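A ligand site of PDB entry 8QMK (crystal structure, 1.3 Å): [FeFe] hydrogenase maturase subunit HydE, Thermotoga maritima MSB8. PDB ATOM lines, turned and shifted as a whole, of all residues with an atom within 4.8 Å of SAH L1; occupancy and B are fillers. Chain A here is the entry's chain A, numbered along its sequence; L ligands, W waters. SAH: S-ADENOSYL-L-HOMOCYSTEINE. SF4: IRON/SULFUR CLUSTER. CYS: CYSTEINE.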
ATOM      1  N   TYR A  79     -33.777 -34.696 -16.512  1.00  0.00           N
ATOM      2  CA  TYR A  79     -33.380 -33.933 -15.308  1.00  0.00           C
ATOM      3  C   TYR A  79     -33.911 -32.501 -15.287  1.00  0.00           C
ATOM      4  O   TYR A  79     -33.865 -31.886 -14.201  1.00  0.00           O
ATOM      5  CB  TYR A  79     -31.820 -33.932 -15.181  1.00  0.00           C
ATOM      6  CG  TYR A  79     -31.123 -33.658 -16.491  1.00  0.00           C
ATOM      7  CD1 TYR A  79     -30.986 -32.333 -16.998  1.00  0.00           C
ATOM      8  CD2 TYR A  79     -30.569 -34.675 -17.265  1.00  0.00           C
ATOM      9  CE1 TYR A  79     -30.347 -32.084 -18.212  1.00  0.00           C
ATOM     10  CE2 TYR A  79     -29.924 -34.432 -18.474  1.00  0.00           C
ATOM     11  CZ  TYR A  79     -29.794 -33.084 -18.918  1.00  0.00           C
ATOM     12  OH  TYR A  79     -29.135 -32.908 -20.146  1.00  0.00           O
ATOM     13  N   CYS A  80     -34.345 -31.967 -16.445  1.00  0.00           N
ATOM     14  CA  CYS A  80     -34.488 -30.484 -16.575  1.00  0.00           C
ATOM     15  C   CYS A  80     -35.924 -30.014 -16.427  1.00  0.00           C
ATOM     16  O   CYS A  80     -36.831 -30.529 -17.107  1.00  0.00           O
ATOM     17  CB  CYS A  80     -33.960 -30.149 -17.955  1.00  0.00           C
ATOM     18  SG  CYS A  80     -33.981 -28.324 -18.261  1.00  0.00           S
ATOM     19  N   GLN A 117     -28.447 -17.670 -23.271  1.00  0.00           N
ATOM     20  CA  GLN A 117     -28.800 -19.073 -23.055  1.00  0.00           C
ATOM     21  C   GLN A 117     -30.311 -19.221 -23.138  1.00  0.00           C
ATOM     22  O   GLN A 117     -31.074 -18.306 -22.763  1.00  0.00           O
ATOM     23  CB  GLN A 117     -28.313 -19.555 -21.685  1.00  0.00           C
ATOM     24  CG  GLN A 117     -28.493 -21.093 -21.504  1.00  0.00           C
ATOM     25  CD  GLN A 117     -27.987 -21.596 -20.191  1.00  0.00           C
ATOM     26  OE1 GLN A 117     -28.727 -21.504 -19.178  1.00  0.00           O
ATOM     27  NE2 GLN A 117     -26.761 -22.071 -20.123  1.00  0.00           N
ATOM     28  N   SER A 118     -30.780 -20.361 -23.645  1.00  0.00           N
ATOM     29  CA  SER A 118     -32.193 -20.628 -23.808  1.00  0.00           C
ATOM     30  C   SER A 118     -32.428 -22.127 -23.803  1.00  0.00           C
ATOM     31  O   SER A 118     -31.518 -22.935 -24.034  1.00  0.00           O
ATOM     32  CB  SER A 118     -32.741 -20.003 -25.055  1.00  0.00           C
ATOM     33  OG  SER A 118     -32.167 -20.512 -26.211  1.00  0.00           O
ATOM     34  N   GLY A 119     -33.697 -22.506 -23.616  1.00  0.00           N
ATOM     35  CA  GLY A 119     -34.152 -23.822 -24.153  1.00  0.00           C
ATOM     36  C   GLY A 119     -33.870 -23.893 -25.654  1.00  0.00           C
ATOM     37  O   GLY A 119     -33.651 -22.848 -26.339  1.00  0.00           O
ATOM     38  N   GLU A 120     -33.964 -25.107 -26.237  1.00  0.00           N
ATOM     39  CA  GLU A 120     -33.866 -25.229 -27.688  1.00  0.00           C
ATOM     40  C   GLU A 120     -35.194 -24.763 -28.302  1.00  0.00           C
ATOM     41  O   GLU A 120     -36.136 -25.555 -28.541  1.00  0.00           O
ATOM     42  CB  GLU A 120     -33.578 -26.679 -28.105  1.00  0.00           C
ATOM     43  CG  GLU A 120     -32.158 -27.112 -27.651  1.00  0.00           C
ATOM     44  CD  GLU A 120     -31.697 -28.349 -28.397  1.00  0.00           C
ATOM     45  OE1 GLU A 120     -32.432 -28.874 -29.277  1.00  0.00           O
ATOM     46  OE2 GLU A 120     -30.600 -28.873 -28.027  1.00  0.00           O
ATOM     47  N   SER A 146     -25.326 -20.304 -25.722  1.00  0.00           N
ATOM     48  CA  SER A 146     -25.572 -21.585 -25.062  1.00  0.00           C
ATOM     49  C   SER A 146     -27.040 -21.977 -25.395  1.00  0.00           C
ATOM     50  O   SER A 146     -27.944 -21.793 -24.616  1.00  0.00           O
ATOM     51  CB  SER A 146     -25.322 -21.400 -23.579  1.00  0.00           C
ATOM     52  OG  SER A 146     -25.473 -22.618 -22.847  1.00  0.00           O
ATOM     53  N   LEU A 147     -27.205 -22.454 -26.635  1.00  0.00           N
ATOM     54  CA  LEU A 147     -28.520 -22.651 -27.226  1.00  0.00           C
ATOM     55  C   LEU A 147     -28.840 -24.127 -27.528  1.00  0.00           C
ATOM     56  O   LEU A 147     -29.928 -24.411 -28.059  1.00  0.00           O
ATOM     57  CB  LEU A 147     -28.658 -21.806 -28.526  1.00  0.00           C
ATOM     58  CG  LEU A 147     -28.179 -20.360 -28.453  1.00  0.00           C
ATOM     59  CD1 LEU A 147     -28.383 -19.680 -29.715  1.00  0.00           C
ATOM     60  CD2 LEU A 147     -28.929 -19.606 -27.334  1.00  0.00           C
ATOM     61  N   GLY A 148     -27.955 -25.020 -27.194  1.00  0.00           N
ATOM     62  CA  GLY A 148     -28.146 -26.457 -27.461  1.00  0.00           C
ATOM     63  C   GLY A 148     -27.600 -26.901 -28.779  1.00  0.00           C
ATOM     64  O   GLY A 148     -26.660 -26.337 -29.341  1.00  0.00           O
ATOM     65  N   LEU A 168     -21.724 -25.751 -24.379  1.00  0.00           N
ATOM     66  CA  LEU A 168     -22.533 -26.934 -24.660  1.00  0.00           C
ATOM     67  C   LEU A 168     -22.056 -28.032 -23.682  1.00  0.00           C
ATOM     68  O   LEU A 168     -21.213 -28.876 -24.017  1.00  0.00           O
ATOM     69  CB  LEU A 168     -22.439 -27.351 -26.116  1.00  0.00           C
ATOM     70  CG  LEU A 168     -23.419 -28.455 -26.529  1.00  0.00           C
ATOM     71  CD1 LEU A 168     -24.823 -27.880 -26.688  1.00  0.00           C
ATOM     72  CD2 LEU A 168     -23.026 -29.028 -27.899  1.00  0.00           C
ATOM     73  N   ARG A 169     -22.546 -27.964 -22.452  1.00  0.00           N
ATOM     74  CA  ARG A 169     -22.080 -28.936 -21.447  1.00  0.00           C
ATOM     75  C   ARG A 169     -22.326 -30.334 -21.935  1.00  0.00           C
ATOM     76  O   ARG A 169     -23.388 -30.605 -22.488  1.00  0.00           O
ATOM     77  CB  ARG A 169     -22.778 -28.672 -20.139  1.00  0.00           C
ATOM     78  CG  ARG A 169     -22.314 -27.262 -19.560  1.00  0.00           C
ATOM     79  CD  ARG A 169     -23.080 -26.720 -18.276  1.00  0.00           C
ATOM     80  NE  ARG A 169     -22.800 -27.601 -17.145  1.00  0.00           N
ATOM     81  CZ  ARG A 169     -23.450 -27.579 -15.980  1.00  0.00           C
ATOM     82  NH1 ARG A 169     -23.202 -28.489 -15.016  1.00  0.00           N
ATOM     83  NH2 ARG A 169     -24.395 -26.627 -15.774  1.00  0.00           N
ATOM     84  N   GLU A 171     -22.709 -33.052 -20.209  1.00  0.00           N
ATOM     85  CA  GLU A 171     -23.660 -33.644 -19.268  1.00  0.00           C
ATOM     86  C   GLU A 171     -23.134 -34.932 -18.611  1.00  0.00           C
ATOM     87  O   GLU A 171     -23.013 -35.021 -17.381  1.00  0.00           O
ATOM     88  CB  GLU A 171     -25.096 -33.890 -19.877  1.00  0.00           C
ATOM     89  CG  GLU A 171     -25.584 -32.654 -20.749  1.00  0.00           C
ATOM     90  CD  GLU A 171     -25.674 -31.354 -20.027  1.00  0.00           C
ATOM     91  OE1 GLU A 171     -25.297 -31.202 -18.861  1.00  0.00           O
ATOM     92  OE2 GLU A 171     -26.201 -30.413 -20.692  1.00  0.00           O
ATOM     93  N   ARG A 182     -31.384 -38.271 -21.919  1.00  0.00           N
ATOM     94  CA  ARG A 182     -31.585 -37.273 -22.994  1.00  0.00           C
ATOM     95  C   ARG A 182     -32.175 -38.017 -24.196  1.00  0.00           C
ATOM     96  O   ARG A 182     -31.471 -38.316 -25.182  1.00  0.00           O
ATOM     97  CB  ARG A 182     -30.293 -36.529 -23.290  1.00  0.00           C
ATOM     98  CG  ARG A 182     -29.624 -35.970 -22.068  1.00  0.00           C
ATOM     99  CD  ARG A 182     -28.435 -35.068 -22.360  1.00  0.00           C
ATOM    100  NE  ARG A 182     -28.920 -33.844 -22.985  1.00  0.00           N
ATOM    101  CZ  ARG A 182     -28.668 -33.431 -24.232  1.00  0.00           C
ATOM    102  NH1 ARG A 182     -27.848 -34.050 -25.035  1.00  0.00           N
ATOM    103  NH2 ARG A 182     -29.391 -32.411 -24.706  1.00  0.00           N
ATOM    104  N   ARG A 190     -23.915 -34.913 -29.289  1.00  0.00           N
ATOM    105  CA  ARG A 190     -23.407 -33.823 -28.440  1.00  0.00           C
ATOM    106  C   ARG A 190     -21.926 -33.567 -28.747  1.00  0.00           C
ATOM    107  O   ARG A 190     -21.457 -32.410 -28.904  1.00  0.00           O
ATOM    108  CB  ARG A 190     -23.583 -34.219 -26.954  1.00  0.00           C
ATOM    109  CG  ARG A 190     -23.447 -33.038 -25.925  1.00  0.00           C
ATOM    110  CD  ARG A 190     -24.702 -32.321 -25.942  1.00  0.00           C
ATOM    111  NE  ARG A 190     -24.835 -31.397 -24.763  1.00  0.00           N
ATOM    112  CZ  ARG A 190     -25.840 -30.520 -24.676  1.00  0.00           C
ATOM    113  NH1 ARG A 190     -26.796 -30.486 -25.583  1.00  0.00           N
ATOM    114  NH2 ARG A 190     -25.808 -29.600 -23.702  1.00  0.00           N
ATOM    115  N   MET A 209     -22.746 -32.787 -15.172  1.00  0.00           N
ATOM    116  CA  MET A 209     -23.412 -32.766 -13.877  1.00  0.00           C
ATOM    117  C   MET A 209     -22.819 -33.881 -13.026  1.00  0.00           C
ATOM    118  O   MET A 209     -22.451 -34.964 -13.565  1.00  0.00           O
ATOM    119  CB  MET A 209     -24.947 -32.904 -14.021  1.00  0.00           C
ATOM    120  CG  MET A 209     -25.601 -31.660 -14.526  1.00  0.00           C
ATOM    121  SD  MET A 209     -27.382 -31.907 -14.871  1.00  0.00           S
ATOM    122  CE  MET A 209     -27.255 -32.782 -16.420  1.00  0.00           C
ATOM    123  N   PRO A 239     -23.551 -29.746  -9.493  1.00  0.00           N
ATOM    124  CA  PRO A 239     -24.293 -30.892  -9.031  1.00  0.00           C
ATOM    125  C   PRO A 239     -25.614 -31.001  -9.786  1.00  0.00           C
ATOM    126  O   PRO A 239     -26.243 -29.990 -10.146  1.00  0.00           O
ATOM    127  CB  PRO A 239     -24.569 -30.562  -7.531  1.00  0.00           C
ATOM    128  CG  PRO A 239     -24.668 -29.020  -7.538  1.00  0.00           C
ATOM    129  CD  PRO A 239     -23.665 -28.607  -8.546  1.00  0.00           C
ATOM    130  N   PHE A 240     -26.092 -32.237  -9.939  1.00  0.00           N
ATOM    131  CA  PHE A 240     -27.497 -32.508 -10.318  1.00  0.00           C
ATOM    132  C   PHE A 240     -28.414 -32.118  -9.186  1.00  0.00           C
ATOM    133  O   PHE A 240     -28.201 -32.572  -8.037  1.00  0.00           O
ATOM    134  CB  PHE A 240     -27.652 -33.999 -10.663  1.00  0.00           C
ATOM    135  CG  PHE A 240     -29.075 -34.465 -10.717  1.00  0.00           C
ATOM    136  CD1 PHE A 240     -29.986 -33.934 -11.595  1.00  0.00           C
ATOM    137  CD2 PHE A 240     -29.533 -35.422  -9.809  1.00  0.00           C
ATOM    138  CE1 PHE A 240     -31.306 -34.343 -11.573  1.00  0.00           C
ATOM    139  CE2 PHE A 240     -30.853 -35.818  -9.835  1.00  0.00           C
ATOM    140  CZ  PHE A 240     -31.698 -35.286 -10.744  1.00  0.00           C
ATOM    141  N   ILE A 241     -29.418 -31.307  -9.475  1.00  0.00           N
ATOM    142  CA  ILE A 241     -30.410 -30.874  -8.484  1.00  0.00           C
ATOM    143  C   ILE A 241     -31.778 -31.399  -8.895  1.00  0.00           C
ATOM    144  O   ILE A 241     -32.334 -30.911  -9.911  1.00  0.00           O
ATOM    145  CB  ILE A 241     -30.391 -29.365  -8.268  1.00  0.00           C
ATOM    146  CG1 ILE A 241     -29.001 -28.945  -7.762  1.00  0.00           C
ATOM    147  CG2 ILE A 241     -31.427 -28.978  -7.274  1.00  0.00           C
ATOM    148  CD1 ILE A 241     -28.778 -27.422  -7.696  1.00  0.00           C
ATOM    149  N   ALA A 280     -25.420 -23.630  -9.938  1.00  0.00           N
ATOM    150  CA  ALA A 280     -25.862 -24.796  -9.126  1.00  0.00           C
ATOM    151  C   ALA A 280     -25.066 -24.991  -7.840  1.00  0.00           C
ATOM    152  O   ALA A 280     -25.614 -25.376  -6.804  1.00  0.00           O
ATOM    153  CB  ALA A 280     -25.873 -26.066 -10.015  1.00  0.00           C
ATOM    154  N   TYR A 313     -37.287 -19.360 -15.348  1.00  0.00           N
ATOM    155  CA  TYR A 313     -36.223 -20.164 -16.001  1.00  0.00           C
ATOM    156  C   TYR A 313     -35.769 -21.257 -15.025  1.00  0.00           C
ATOM    157  O   TYR A 313     -34.639 -21.274 -14.506  1.00  0.00           O
ATOM    158  CB  TYR A 313     -35.082 -19.253 -16.472  1.00  0.00           C
ATOM    159  CG  TYR A 313     -34.127 -19.957 -17.431  1.00  0.00           C
ATOM    160  CD1 TYR A 313     -34.452 -20.136 -18.797  1.00  0.00           C
ATOM    161  CD2 TYR A 313     -32.859 -20.374 -16.975  1.00  0.00           C
ATOM    162  CE1 TYR A 313     -33.557 -20.706 -19.690  1.00  0.00           C
ATOM    163  CE2 TYR A 313     -31.948 -20.951 -17.834  1.00  0.00           C
ATOM    164  CZ  TYR A 313     -32.274 -21.131 -19.200  1.00  0.00           C
ATOM    165  OH  TYR A 313     -31.362 -21.653 -20.077  1.00  0.00           O
ATOM    166  N   LEU A 315     -34.683 -24.362 -14.249  1.00  0.00           N
ATOM    167  CA  LEU A 315     -33.959 -25.597 -14.587  1.00  0.00           C
ATOM    168  C   LEU A 315     -34.041 -26.585 -13.434  1.00  0.00           C
ATOM    169  O   LEU A 315     -34.207 -27.796 -13.641  1.00  0.00           O
ATOM    170  CB  LEU A 315     -32.473 -25.293 -14.815  1.00  0.00           C
ATOM    171  CG  LEU A 315     -32.137 -24.338 -15.898  1.00  0.00           C
ATOM    172  CD1 LEU A 315     -30.625 -24.131 -15.937  1.00  0.00           C
ATOM    173  CD2 LEU A 315     -32.533 -24.809 -17.296  1.00  0.00           C
ATOM    174  N   TYR A 316     -33.944 -26.072 -12.203  1.00  0.00           N
ATOM    175  CA  TYR A 316     -33.957 -26.832 -10.966  1.00  0.00           C
ATOM    176  C   TYR A 316     -34.469 -25.930  -9.852  1.00  0.00           C
ATOM    177  O   TYR A 316     -34.317 -24.687  -9.936  1.00  0.00           O
ATOM    178  CB  TYR A 316     -32.549 -27.395 -10.597  1.00  0.00           C
ATOM    179  CG  TYR A 316     -31.406 -26.454 -10.792  1.00  0.00           C
ATOM    180  CD1 TYR A 316     -31.123 -25.493  -9.781  1.00  0.00           C
ATOM    181  CD2 TYR A 316     -30.621 -26.430 -11.919  1.00  0.00           C
ATOM    182  CE1 TYR A 316     -30.063 -24.585  -9.962  1.00  0.00           C
ATOM    183  CE2 TYR A 316     -29.554 -25.519 -12.085  1.00  0.00           C
ATOM    184  CZ  TYR A 316     -29.351 -24.570 -11.060  1.00  0.00           C
ATOM    185  OH  TYR A 316     -28.281 -23.696 -11.279  1.00  0.00           O
HETATM  186  N   SAH L   1     -30.686 -26.064 -23.775  1.00  0.00           N
HETATM  187  CA  SAH L   1     -29.246 -25.743 -23.648  1.00  0.00           C
HETATM  188  CB  SAH L   1     -28.975 -24.594 -22.618  1.00  0.00           C
HETATM  189  CG  SAH L   1     -29.925 -24.548 -21.421  1.00  0.00           C
HETATM  190  SD  SAH L   1     -29.854 -25.894 -20.256  1.00  0.00           S
HETATM  191  C   SAH L   1     -28.528 -27.058 -23.353  1.00  0.00           C
HETATM  192  O   SAH L   1     -27.277 -27.027 -23.502  1.00  0.00           O
HETATM  193  OXT SAH L   1     -29.144 -28.037 -22.860  1.00  0.00           O
HETATM  194  C5' SAH L   1     -28.213 -25.448 -19.445  1.00  0.00           C
HETATM  195  C4' SAH L   1     -27.653 -26.512 -18.480  1.00  0.00           C
HETATM  196  O4' SAH L   1     -28.429 -26.624 -17.281  1.00  0.00           O
HETATM  197  C3' SAH L   1     -27.489 -27.964 -18.980  1.00  0.00           C
HETATM  198  O3' SAH L   1     -26.291 -28.047 -19.773  1.00  0.00           O
HETATM  199  C2' SAH L   1     -27.384 -28.748 -17.683  1.00  0.00           C
HETATM  200  O2' SAH L   1     -26.083 -29.112 -17.317  1.00  0.00           O
HETATM  201  C1' SAH L   1     -27.959 -27.796 -16.588  1.00  0.00           C
HETATM  202  N9  SAH L   1     -29.101 -28.371 -15.852  1.00  0.00           N
HETATM  203  C8  SAH L   1     -30.323 -28.683 -16.399  1.00  0.00           C
HETATM  204  N7  SAH L   1     -31.099 -29.314 -15.480  1.00  0.00           N
HETATM  205  C5  SAH L   1     -30.357 -29.389 -14.309  1.00  0.00           C
HETATM  206  C6  SAH L   1     -30.619 -29.917 -13.067  1.00  0.00           C
HETATM  207  N6  SAH L   1     -31.765 -30.527 -12.678  1.00  0.00           N
HETATM  208  N1  SAH L   1     -29.619 -29.864 -12.132  1.00  0.00           N
HETATM  209  C2  SAH L   1     -28.441 -29.230 -12.424  1.00  0.00           C
HETATM  210  N3  SAH L   1     -28.142 -28.677 -13.624  1.00  0.00           N
HETATM  211  C4  SAH L   1     -29.107 -28.782 -14.590  1.00  0.00           C
HETATM  212 FE1  SF4 L   2     -33.310 -28.446 -20.471  1.00  0.00          FE
HETATM  213 FE2  SF4 L   2     -33.981 -28.328 -23.081  1.00  0.00          FE
HETATM  214 FE3  SF4 L   2     -32.494 -30.414 -22.163  1.00  0.00          FE
HETATM  215 FE4  SF4 L   2     -31.255 -27.782 -22.349  1.00  0.00          FE
HETATM  216  S1  SF4 L   2     -32.093 -29.244 -24.056  1.00  0.00           S
HETATM  217  S2  SF4 L   2     -31.191 -29.321 -20.585  1.00  0.00           S
HETATM  218  S3  SF4 L   2     -33.247 -26.606 -21.764  1.00  0.00           S
HETATM  219  S4  SF4 L   2     -34.701 -29.925 -21.627  1.00  0.00           S
HETATM  220  N   CYS L   3     -25.968 -21.613 -15.265  1.00  0.00           N
HETATM  221  CA  CYS L   3     -26.721 -22.811 -14.943  1.00  0.00           C
HETATM  222  C   CYS L   3     -25.847 -23.567 -14.015  1.00  0.00           C
HETATM  223  O   CYS L   3     -24.616 -23.476 -14.367  1.00  0.00           O
HETATM  224  CB  CYS L   3     -26.959 -23.637 -16.221  1.00  0.00           C
HETATM  225  SG  CYS L   3     -25.443 -23.709 -17.203  1.00  0.00           S
HETATM  226  OXT CYS L   3     -26.280 -24.333 -13.183  1.00  0.00           O
HETATM  227  O   HOH W   1     -29.227 -29.088 -25.673  1.00  0.00           O
HETATM  228  O   HOH W   2     -25.990 -25.054 -25.016  1.00  0.00           O
HETATM  229  O   HOH W   3     -28.608 -30.893 -21.851  1.00  0.00           O
HETATM  230  O   HOH W   4     -25.054 -26.540 -21.754  1.00  0.00           O
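O of Ile 241 is in hydrogen-bond range of N6 of SAH L1 (2.9 Å).
The side-chain amide nitrogen (NE2) of Gln 117 sits close to a sulfur (SG) of CYS L3, 3.6 Å away.
OH of Tyr 316 is in hydrogen-bond range of OXT of CYS L3.
A nitrogen (N) of SAH L1 lies close to the backbone carbonyl oxygen (O) of Ser 118, at 3.2 Å.
N1 of SAH L1 sits at hydrogen-bond distance from N of Ile 241 (3.0 Å).
The guanidinium group (NH2) of Arg 190 is in salt-bridge range of an oxygen (O) of SAH L1.
The backbone NH of Ala 280 sits at hydrogen-bond distance from an oxygen (OXT) of CYS L3, 3.4 Å away.
O of Tyr 79 sits at hydrogen-bond distance from N6 of SAH L1, at 2.9 Å.
NH2 of Arg 169 lies within salt-bridge range of OXT of CYS L3 (3.9 Å).
An oxygen (O2') of SAH L1 sits close to the guanidinium group of Arg 169 (3.4 Å).
An iron atom (FE1) of SF4 L2 is bound by the side-chain sulfur (SG) of Cys 80 (2.3 Å).
The side-chain carboxylate (OE2) of Glu 171 is in hydrogen-bond range of an oxygen (O3') of SAH L1 (2.5 Å).
A nitrogen (N3) of SAH L1 sits close to the side-chain sulfur of Met 209 (3.5 Å).
Cys 80 touches SAH L1.
Gln 117 touches SAH L1.
O of Ser 146 touches CB of SAH L1 (3.6 Å).
Gly 148 touches SAH L1 (N to CA, 3.8 Å).
Pro 239 touches SAH L1 (O to C2, 3.3 Å).
CA of Phe 240 touches N1 of SAH L1, at 3.8 Å.
OH of Tyr 313 touches CG of SAH L1, at 3.5 Å.
Leu 315 touches SAH L1.
CD2 of Tyr 316 touches N1 of SAH L1, at 3.6 Å.
Within 4 Å of SAH L1: Tyr 79, Cys 80, Gln 117, Ser 118, Ser 146, Gly 148, Arg 169, Glu 171, Arg 190, Met 209, Pro 239, Phe 240, Ile 241, Tyr 313, Leu 315 and Tyr 316.
Along chain A the residues within 4 Å of SAH L1 span positions 79 to 316.
The nearest printed residue that does not touch SAH L1 is Leu 168 (4.1 Å).
The backbone NH of Ala 280 lies within hydrogen-bond range of the side-chain hydroxyl of Tyr 316.
O of Arg 169 lies within hydrogen-bond range of NE of Arg 190.
The side-chain hydroxyl (OH) of Tyr 79 lies within hydrogen-bond range of the guanidinium group (NE) of Arg 182, at 3.0 Å.
The side-chain hydroxyl (OH) of Tyr 313 is in hydrogen-bond range of the side-chain amide oxygen (OE1) of Gln 117 (2.8 Å).
O of Glu 171 sits at hydrogen-bond distance from N of Met 209, 3.2 Å away.
OG of Ser 146 is in hydrogen-bond range of NE2 of Gln 117 (3.1 Å).
The side-chain carboxylate of Glu 171 lies within salt-bridge range of the guanidinium group of Arg 190, at 3.1 Å.
The backbone NH (N) of Ser 118 is in hydrogen-bond range of the backbone carbonyl oxygen (O) of Ser 146.
Water W4 bridges O3' of SAH L1 (2.8 Å) and N of Arg 169 (3.0 Å).
Water W2 lies within hydrogen-bond range of O of SAH L1, N of Gly 148, N of Leu 147 and OG of Ser 146.
Water W1 lies within hydrogen-bond range of the side-chain carboxylate of Glu 120 (2.7 Å), the guanidinium group of Arg 190 (2.8 Å), a sulfur (S1) of SF4 L2 (3.3 Å) and the guanidinium group of Arg 182 (3.5 Å).
Water W3 lies within hydrogen-bond range of the side-chain hydroxyl (OH) of Tyr 79 (2.7 Å), the side-chain carboxylate (OE2) of Glu 171 (2.7 Å), the guanidinium group (NE) of Arg 182 (3.2 Å) and a sulfur (S2) of SF4 L2 (3.3 Å).
An oxygen (OXT) of SAH L1 binds an iron atom (FE4) of SF4 L2.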
